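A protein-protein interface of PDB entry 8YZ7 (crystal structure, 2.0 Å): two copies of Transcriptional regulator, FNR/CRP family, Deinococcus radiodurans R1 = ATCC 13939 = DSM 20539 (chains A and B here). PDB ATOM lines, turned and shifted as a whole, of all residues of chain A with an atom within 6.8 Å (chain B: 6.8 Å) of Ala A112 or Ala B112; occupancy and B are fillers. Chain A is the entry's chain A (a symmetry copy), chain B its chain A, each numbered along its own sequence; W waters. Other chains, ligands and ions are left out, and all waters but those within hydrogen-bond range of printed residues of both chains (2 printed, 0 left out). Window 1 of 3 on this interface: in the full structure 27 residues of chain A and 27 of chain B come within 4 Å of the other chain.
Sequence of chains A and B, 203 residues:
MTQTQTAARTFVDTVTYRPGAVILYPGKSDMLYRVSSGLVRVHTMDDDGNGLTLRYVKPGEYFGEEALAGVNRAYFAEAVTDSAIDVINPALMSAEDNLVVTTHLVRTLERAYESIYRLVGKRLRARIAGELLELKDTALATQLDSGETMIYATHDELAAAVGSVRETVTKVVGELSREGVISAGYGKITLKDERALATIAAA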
ATOM      1  N   LEU A  54      22.333  16.615  22.083  1.00  0.00           N
ATOM      2  CA  LEU A  54      21.969  16.378  20.689  1.00  0.00           C
ATOM      3  C   LEU A  54      20.460  16.222  20.527  1.00  0.00           C
ATOM      4  O   LEU A  54      19.873  16.744  19.569  1.00  0.00           O
ATOM      5  CB  LEU A  54      22.681  15.133  20.165  1.00  0.00           C
ATOM      6  CG  LEU A  54      24.195  15.258  20.277  1.00  0.00           C
ATOM      7  CD1 LEU A  54      24.887  13.949  19.871  1.00  0.00           C
ATOM      8  CD2 LEU A  54      24.648  16.421  19.422  1.00  0.00           C
ATOM      9  N   ARG A 107      11.904  10.688  11.393  1.00  0.00           N
ATOM     10  CA  ARG A 107      11.499  11.811  12.233  1.00  0.00           C
ATOM     11  C   ARG A 107      12.672  12.355  13.024  1.00  0.00           C
ATOM     12  O   ARG A 107      12.789  13.568  13.222  1.00  0.00           O
ATOM     13  CB  ARG A 107      10.392  11.393  13.188  1.00  0.00           C
ATOM     14  CG  ARG A 107       9.198  10.859  12.468  1.00  0.00           C
ATOM     15  CD  ARG A 107       8.221  10.292  13.459  1.00  0.00           C
ATOM     16  NE  ARG A 107       7.109   9.650  12.777  1.00  0.00           N
ATOM     17  CZ  ARG A 107       6.102  10.298  12.209  1.00  0.00           C
ATOM     18  NH1 ARG A 107       6.029  11.622  12.235  1.00  0.00           N
ATOM     19  NH2 ARG A 107       5.142   9.603  11.604  1.00  0.00           N
ATOM     20  N   THR A 108      13.539  11.467  13.510  1.00  0.00           N
ATOM     21  CA  THR A 108      14.671  11.936  14.294  1.00  0.00           C
ATOM     22  C   THR A 108      15.622  12.758  13.430  1.00  0.00           C
ATOM     23  O   THR A 108      16.145  13.787  13.876  1.00  0.00           O
ATOM     24  CB  THR A 108      15.395  10.755  14.937  1.00  0.00           C
ATOM     25  OG1 THR A 108      14.473  10.014  15.751  1.00  0.00           O
ATOM     26  CG2 THR A 108      16.518  11.251  15.826  1.00  0.00           C
ATOM     27  N   LEU A 109      15.831  12.343  12.178  1.00  0.00           N
ATOM     28  CA  LEU A 109      16.676  13.132  11.284  1.00  0.00           C
ATOM     29  C   LEU A 109      16.029  14.472  10.967  1.00  0.00           C
ATOM     30  O   LEU A 109      16.720  15.494  10.852  1.00  0.00           O
ATOM     31  CB  LEU A 109      16.954  12.358   9.996  1.00  0.00           C
ATOM     32  CG  LEU A 109      17.838  13.083   8.980  1.00  0.00           C
ATOM     33  CD1 LEU A 109      19.251  13.246   9.532  1.00  0.00           C
ATOM     34  CD2 LEU A 109      17.862  12.341   7.662  1.00  0.00           C
ATOM     35  N   GLU A 110      14.702  14.492  10.818  1.00  0.00           N
ATOM     36  CA  GLU A 110      14.025  15.765  10.588  1.00  0.00           C
ATOM     37  C   GLU A 110      14.229  16.710  11.764  1.00  0.00           C
ATOM     38  O   GLU A 110      14.428  17.916  11.570  1.00  0.00           O
ATOM     39  CB  GLU A 110      12.532  15.543  10.322  1.00  0.00           C
ATOM     40  CG  GLU A 110      11.800  16.828   9.937  1.00  0.00           C
ATOM     41  CD  GLU A 110      10.286  16.666   9.874  1.00  0.00           C
ATOM     42  OE1 GLU A 110       9.787  15.576  10.245  1.00  0.00           O
ATOM     43  OE2 GLU A 110       9.601  17.636   9.458  1.00  0.00           O
ATOM     44  N   ARG A 111      14.208  16.180  12.994  1.00  0.00           N
ATOM     45  CA  ARG A 111      14.463  17.004  14.174  1.00  0.00           C
ATOM     46  C   ARG A 111      15.917  17.463  14.237  1.00  0.00           C
ATOM     47  O   ARG A 111      16.211  18.567  14.721  1.00  0.00           O
ATOM     48  CB  ARG A 111      14.108  16.231  15.453  1.00  0.00           C
ATOM     49  CG  ARG A 111      12.603  16.018  15.708  1.00  0.00           C
ATOM     50  CD  ARG A 111      12.368  14.813  16.645  1.00  0.00           C
ATOM     51  NE  ARG A 111      12.527  15.163  18.051  1.00  0.00           N
ATOM     52  CZ  ARG A 111      13.512  14.753  18.843  1.00  0.00           C
ATOM     53  NH1 ARG A 111      14.467  13.941  18.403  1.00  0.00           N
ATOM     54  NH2 ARG A 111      13.543  15.174  20.108  1.00  0.00           N
ATOM     55  N   ALA A 112      16.845  16.621  13.791  1.00  0.00           N
ATOM     56  CA  ALA A 112      18.241  17.051  13.737  1.00  0.00           C
ATOM     57  C   ALA A 112      18.415  18.222  12.775  1.00  0.00           C
ATOM     58  O   ALA A 112      19.122  19.187  13.082  1.00  0.00           O
ATOM     59  CB  ALA A 112      19.134  15.881  13.329  1.00  0.00           C
ATOM     60  N   TYR A 113      17.750  18.175  11.617  1.00  0.00           N
ATOM     61  CA  TYR A 113      17.875  19.281  10.671  1.00  0.00           C
ATOM     62  C   TYR A 113      17.225  20.550  11.202  1.00  0.00           C
ATOM     63  O   TYR A 113      17.719  21.662  10.957  1.00  0.00           O
ATOM     64  CB  TYR A 113      17.280  18.898   9.320  1.00  0.00           C
ATOM     65  CG  TYR A 113      18.188  17.936   8.601  1.00  0.00           C
ATOM     66  CD1 TYR A 113      19.508  17.790   9.011  1.00  0.00           C
ATOM     67  CD2 TYR A 113      17.739  17.165   7.547  1.00  0.00           C
ATOM     68  CE1 TYR A 113      20.361  16.909   8.384  1.00  0.00           C
ATOM     69  CE2 TYR A 113      18.590  16.283   6.906  1.00  0.00           C
ATOM     70  CZ  TYR A 113      19.895  16.160   7.332  1.00  0.00           C
ATOM     71  OH  TYR A 113      20.737  15.276   6.693  1.00  0.00           O
ATOM     72  N   GLU A 114      16.112  20.416  11.924  1.00  0.00           N
ATOM     73  CA  GLU A 114      15.526  21.604  12.529  1.00  0.00           C
ATOM     74  C   GLU A 114      16.467  22.201  13.570  1.00  0.00           C
ATOM     75  O   GLU A 114      16.594  23.430  13.669  1.00  0.00           O
ATOM     76  CB  GLU A 114      14.173  21.268  13.152  1.00  0.00           C
ATOM     77  CG  GLU A 114      13.501  22.471  13.762  1.00  0.00           C
ATOM     78  CD  GLU A 114      12.209  22.101  14.462  1.00  0.00           C
ATOM     79  OE1 GLU A 114      11.897  20.884  14.490  1.00  0.00           O
ATOM     80  OE2 GLU A 114      11.516  23.014  14.976  1.00  0.00           O
ATOM     81  N   SER A 115      17.145  21.345  14.345  1.00  0.00           N
ATOM     82  CA  SER A 115      18.128  21.826  15.316  1.00  0.00           C
ATOM     83  C   SER A 115      19.220  22.636  14.635  1.00  0.00           C
ATOM     84  O   SER A 115      19.620  23.701  15.121  1.00  0.00           O
ATOM     85  CB  SER A 115      18.747  20.649  16.078  1.00  0.00           C
ATOM     86  OG  SER A 115      17.810  20.040  16.949  1.00  0.00           O
ATOM     87  N   ILE A 116      19.724  22.132  13.508  1.00  0.00           N
ATOM     88  CA  ILE A 116      20.740  22.848  12.747  1.00  0.00           C
ATOM     89  C   ILE A 116      20.214  24.203  12.297  1.00  0.00           C
ATOM     90  O   ILE A 116      20.846  25.242  12.523  1.00  0.00           O
ATOM     91  CB  ILE A 116      21.188  22.000  11.543  1.00  0.00           C
ATOM     92  CG1 ILE A 116      21.955  20.769  12.039  1.00  0.00           C
ATOM     93  CG2 ILE A 116      21.993  22.840  10.577  1.00  0.00           C
ATOM     94  CD1 ILE A 116      22.241  19.762  10.946  1.00  0.00           C
ATOM     95  N   TYR A 117      19.073  24.205  11.611  1.00  0.00           N
ATOM     96  CA  TYR A 117      18.487  25.457  11.142  1.00  0.00           C
ATOM     97  C   TYR A 117      18.421  26.482  12.271  1.00  0.00           C
ATOM     98  O   TYR A 117      18.831  27.640  12.106  1.00  0.00           O
ATOM     99  CB  TYR A 117      17.091  25.186  10.566  1.00  0.00           C
ATOM    100  CG  TYR A 117      16.275  26.435  10.297  1.00  0.00           C
ATOM    101  CD1 TYR A 117      16.631  27.309   9.274  1.00  0.00           C
ATOM    102  CD2 TYR A 117      15.149  26.738  11.062  1.00  0.00           C
ATOM    103  CE1 TYR A 117      15.896  28.457   9.022  1.00  0.00           C
ATOM    104  CE2 TYR A 117      14.398  27.887  10.813  1.00  0.00           C
ATOM    105  CZ  TYR A 117      14.780  28.738   9.792  1.00  0.00           C
ATOM    106  OH  TYR A 117      14.050  29.878   9.536  1.00  0.00           O
ATOM    107  N   LEU B  54      22.020  21.610   4.616  1.00  0.00           N
ATOM    108  CA  LEU B  54      21.873  20.604   5.664  1.00  0.00           C
ATOM    109  C   LEU B  54      22.839  19.441   5.458  1.00  0.00           C
ATOM    110  O   LEU B  54      23.434  18.940   6.422  1.00  0.00           O
ATOM    111  CB  LEU B  54      20.436  20.088   5.697  1.00  0.00           C
ATOM    112  CG  LEU B  54      19.436  21.213   5.933  1.00  0.00           C
ATOM    113  CD1 LEU B  54      17.994  20.698   5.831  1.00  0.00           C
ATOM    114  CD2 LEU B  54      19.717  21.832   7.286  1.00  0.00           C
ATOM    115  N   ARG B 107      23.737   6.370   9.409  1.00  0.00           N
ATOM    116  CA  ARG B 107      24.928   7.156   9.101  1.00  0.00           C
ATOM    117  C   ARG B 107      24.577   8.612   8.867  1.00  0.00           C
ATOM    118  O   ARG B 107      25.330   9.511   9.257  1.00  0.00           O
ATOM    119  CB  ARG B 107      25.633   6.601   7.875  1.00  0.00           C
ATOM    120  CG  ARG B 107      26.018   5.167   8.047  1.00  0.00           C
ATOM    121  CD  ARG B 107      26.538   4.623   6.746  1.00  0.00           C
ATOM    122  NE  ARG B 107      26.797   3.196   6.851  1.00  0.00           N
ATOM    123  CZ  ARG B 107      27.855   2.669   7.454  1.00  0.00           C
ATOM    124  NH1 ARG B 107      28.786   3.432   8.009  1.00  0.00           N
ATOM    125  NH2 ARG B 107      27.984   1.346   7.496  1.00  0.00           N
ATOM    126  N   THR B 108      23.450   8.866   8.205  1.00  0.00           N
ATOM    127  CA  THR B 108      23.079  10.247   7.936  1.00  0.00           C
ATOM    128  C   THR B 108      22.770  10.985   9.234  1.00  0.00           C
ATOM    129  O   THR B 108      23.150  12.150   9.400  1.00  0.00           O
ATOM    130  CB  THR B 108      21.890  10.298   6.979  1.00  0.00           C
ATOM    131  OG1 THR B 108      22.223   9.606   5.765  1.00  0.00           O
ATOM    132  CG2 THR B 108      21.563  11.737   6.628  1.00  0.00           C
ATOM    133  N   LEU B 109      22.113  10.313  10.183  1.00  0.00           N
ATOM    134  CA  LEU B 109      21.854  10.947  11.474  1.00  0.00           C
ATOM    135  C   LEU B 109      23.152  11.188  12.232  1.00  0.00           C
ATOM    136  O   LEU B 109      23.302  12.210  12.916  1.00  0.00           O
ATOM    137  CB  LEU B 109      20.904  10.088  12.307  1.00  0.00           C
ATOM    138  CG  LEU B 109      20.552  10.656  13.683  1.00  0.00           C
ATOM    139  CD1 LEU B 109      19.732  11.933  13.532  1.00  0.00           C
ATOM    140  CD2 LEU B 109      19.803   9.635  14.511  1.00  0.00           C
ATOM    141  N   GLU B 110      24.104  10.257  12.127  1.00  0.00           N
ATOM    142  CA  GLU B 110      25.395  10.476  12.772  1.00  0.00           C
ATOM    143  C   GLU B 110      26.087  11.707  12.202  1.00  0.00           C
ATOM    144  O   GLU B 110      26.702  12.479  12.947  1.00  0.00           O
ATOM    145  CB  GLU B 110      26.287   9.237  12.632  1.00  0.00           C
ATOM    146  CG  GLU B 110      27.597   9.358  13.408  1.00  0.00           C
ATOM    147  CD  GLU B 110      28.582   8.233  13.113  1.00  0.00           C
ATOM    148  OE1 GLU B 110      28.294   7.411  12.209  1.00  0.00           O
ATOM    149  OE2 GLU B 110      29.644   8.180  13.784  1.00  0.00           O
ATOM    150  N   ARG B 111      25.978  11.922  10.885  1.00  0.00           N
ATOM    151  CA  ARG B 111      26.554  13.116  10.267  1.00  0.00           C
ATOM    152  C   ARG B 111      25.810  14.381  10.684  1.00  0.00           C
ATOM    153  O   ARG B 111      26.413  15.458  10.808  1.00  0.00           O
ATOM    154  CB  ARG B 111      26.537  12.986   8.737  1.00  0.00           C
ATOM    155  CG  ARG B 111      27.540  11.978   8.141  1.00  0.00           C
ATOM    156  CD  ARG B 111      27.087  11.514   6.739  1.00  0.00           C
ATOM    157  NE  ARG B 111      27.461  12.458   5.693  1.00  0.00           N
ATOM    158  CZ  ARG B 111      26.619  13.215   4.999  1.00  0.00           C
ATOM    159  NH1 ARG B 111      25.307  13.159   5.197  1.00  0.00           N
ATOM    160  NH2 ARG B 111      27.107  14.055   4.085  1.00  0.00           N
ATOM    161  N   ALA B 112      24.496  14.286  10.869  1.00  0.00           N
ATOM    162  CA  ALA B 112      23.753  15.443  11.366  1.00  0.00           C
ATOM    163  C   ALA B 112      24.222  15.835  12.762  1.00  0.00           C
ATOM    164  O   ALA B 112      24.401  17.021  13.055  1.00  0.00           O
ATOM    165  CB  ALA B 112      22.255  15.143  11.364  1.00  0.00           C
ATOM    166  N   TYR B 113      24.463  14.850  13.634  1.00  0.00           N
ATOM    167  CA  TYR B 113      24.928  15.177  14.978  1.00  0.00           C
ATOM    168  C   TYR B 113      26.337  15.752  14.962  1.00  0.00           C
ATOM    169  O   TYR B 113      26.665  16.639  15.763  1.00  0.00           O
ATOM    170  CB  TYR B 113      24.860  13.950  15.881  1.00  0.00           C
ATOM    171  CG  TYR B 113      23.431  13.647  16.248  1.00  0.00           C
ATOM    172  CD1 TYR B 113      22.449  14.614  16.067  1.00  0.00           C
ATOM    173  CD2 TYR B 113      23.056  12.415  16.744  1.00  0.00           C
ATOM    174  CE1 TYR B 113      21.131  14.365  16.378  1.00  0.00           C
ATOM    175  CE2 TYR B 113      21.736  12.156  17.067  1.00  0.00           C
ATOM    176  CZ  TYR B 113      20.782  13.134  16.880  1.00  0.00           C
ATOM    177  OH  TYR B 113      19.468  12.872  17.198  1.00  0.00           O
ATOM    178  N   GLU B 114      27.192  15.259  14.065  1.00  0.00           N
ATOM    179  CA  GLU B 114      28.513  15.860  13.958  1.00  0.00           C
ATOM    180  C   GLU B 114      28.414  17.306  13.487  1.00  0.00           C
ATOM    181  O   GLU B 114      29.151  18.176  13.972  1.00  0.00           O
ATOM    182  CB  GLU B 114      29.392  15.042  13.014  1.00  0.00           C
ATOM    183  CG  GLU B 114      30.787  15.597  12.894  1.00  0.00           C
ATOM    184  CD  GLU B 114      31.613  14.833  11.877  1.00  0.00           C
ATOM    185  OE1 GLU B 114      31.043  13.905  11.252  1.00  0.00           O
ATOM    186  OE2 GLU B 114      32.815  15.157  11.708  1.00  0.00           O
ATOM    187  N   SER B 115      27.497  17.584  12.549  1.00  0.00           N
ATOM    188  CA  SER B 115      27.279  18.957  12.096  1.00  0.00           C
ATOM    189  C   SER B 115      26.892  19.862  13.255  1.00  0.00           C
ATOM    190  O   SER B 115      27.393  20.987  13.378  1.00  0.00           O
ATOM    191  CB  SER B 115      26.191  18.995  11.016  1.00  0.00           C
ATOM    192  OG  SER B 115      26.631  18.399   9.809  1.00  0.00           O
ATOM    193  N   ILE B 116      25.985  19.388  14.109  1.00  0.00           N
ATOM    194  CA  ILE B 116      25.578  20.150  15.282  1.00  0.00           C
ATOM    195  C   ILE B 116      26.773  20.420  16.184  1.00  0.00           C
ATOM    196  O   ILE B 116      27.040  21.566  16.567  1.00  0.00           O
ATOM    197  CB  ILE B 116      24.470  19.396  16.040  1.00  0.00           C
ATOM    198  CG1 ILE B 116      23.190  19.381  15.196  1.00  0.00           C
ATOM    199  CG2 ILE B 116      24.261  20.003  17.409  1.00  0.00           C
ATOM    200  CD1 ILE B 116      22.116  18.473  15.757  1.00  0.00           C
ATOM    201  N   TYR B 117      27.479  19.362  16.576  1.00  0.00           N
ATOM    202  CA  TYR B 117      28.646  19.521  17.438  1.00  0.00           C
ATOM    203  C   TYR B 117      29.578  20.601  16.897  1.00  0.00           C
ATOM    204  O   TYR B 117      30.014  21.497  17.634  1.00  0.00           O
ATOM    205  CB  TYR B 117      29.377  18.179  17.565  1.00  0.00           C
ATOM    206  CG  TYR B 117      30.747  18.274  18.209  1.00  0.00           C
ATOM    207  CD1 TYR B 117      30.877  18.579  19.561  1.00  0.00           C
ATOM    208  CD2 TYR B 117      31.907  18.055  17.467  1.00  0.00           C
ATOM    209  CE1 TYR B 117      32.123  18.675  20.159  1.00  0.00           C
ATOM    210  CE2 TYR B 117      33.167  18.142  18.060  1.00  0.00           C
ATOM    211  CZ  TYR B 117      33.263  18.452  19.404  1.00  0.00           C
ATOM    212  OH  TYR B 117      34.500  18.544  20.004  1.00  0.00           O
HETATM  213  O   HOH W   1      17.390  14.492  16.462  1.00  0.00           O
HETATM  214  O   HOH W   2      23.184  14.554   7.680  1.00  0.00           O
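Leu A109 touches Ala B112, and with the chains exchanged Ala A112 touches Leu B109.
Ala B112 touches its own counterpart, Ala A112.
Ala A112 touches Tyr B113, and with the chains exchanged Tyr A113 touches Ala B112.
Ile B116 touches its own counterpart, Ile A116.
12 positions are printed for both chains.
Tyr B113 touches Leu A54 (CG to CD1, 3.9 Å).
Leu B109 touches Thr A108 (CD2 to CG2, 3.9 Å).
Tyr B113 touches Thr A108.
Leu A109 touches Leu B109 (CA to CD1, 3.98 Å).
CD1 of Leu A109 touches CB of Ala B112, 3.997 Å away.
Leu B109 touches Ala A112 (CD1 to CB, 3.998 Å).
Leu B54 touches Tyr A113 (CD1 to CG, 3.9 Å).
Tyr A113 touches Thr B108.
Tyr A113 touches Ala B112.
CG1 of Ile B116 touches CG1 of Ile A116, at 3.7 Å.
Of the printed residues of chain B, Leu A54 touches Tyr B113.
Printed residues of chain B within 4 Å of Leu A109: Thr B108, Leu B109 and Ala B112.
Of the printed residues of chain B, Ala A112 touches Leu B109 (3.998 Å), Ala B112 (3.8 Å) and Tyr B113 (3.9 Å).
Tyr A117 touches none of the printed residues of chain B.
Of the printed residues of chain A, Leu B109 touches Thr A108 (3.9 Å), Leu A109 (3.98 Å) and Ala A112 (3.998 Å).
Arg B111 touches none of the printed residues of chain A.
Printed residues of chain A within 4 Å of Ala B112: Leu A109, Ala A112 and Tyr A113.
The nearest printed residue of chain A that does not touch Ala B112 is Ile A116 (4.1 Å).
Hydrophobic or aromatic side chains of chain B within 4 Å of the printed part of chain A: Leu B54, Leu B109, Ala B112, Tyr B113 and Ile B116.
Among the printed residues, 13 pairs touch across the chains.
Water W2 lies within hydrogen-bond range of OH of Tyr A113 (2.7 Å), O of Thr B108 (3.0 Å) and N of Ala B112 (3.5 Å).
Water W1 lies within hydrogen-bond range of OH of Tyr B113 (2.7 Å), O of Thr A108 (3.0 Å) and N of Ala A112 (3.5 Å).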
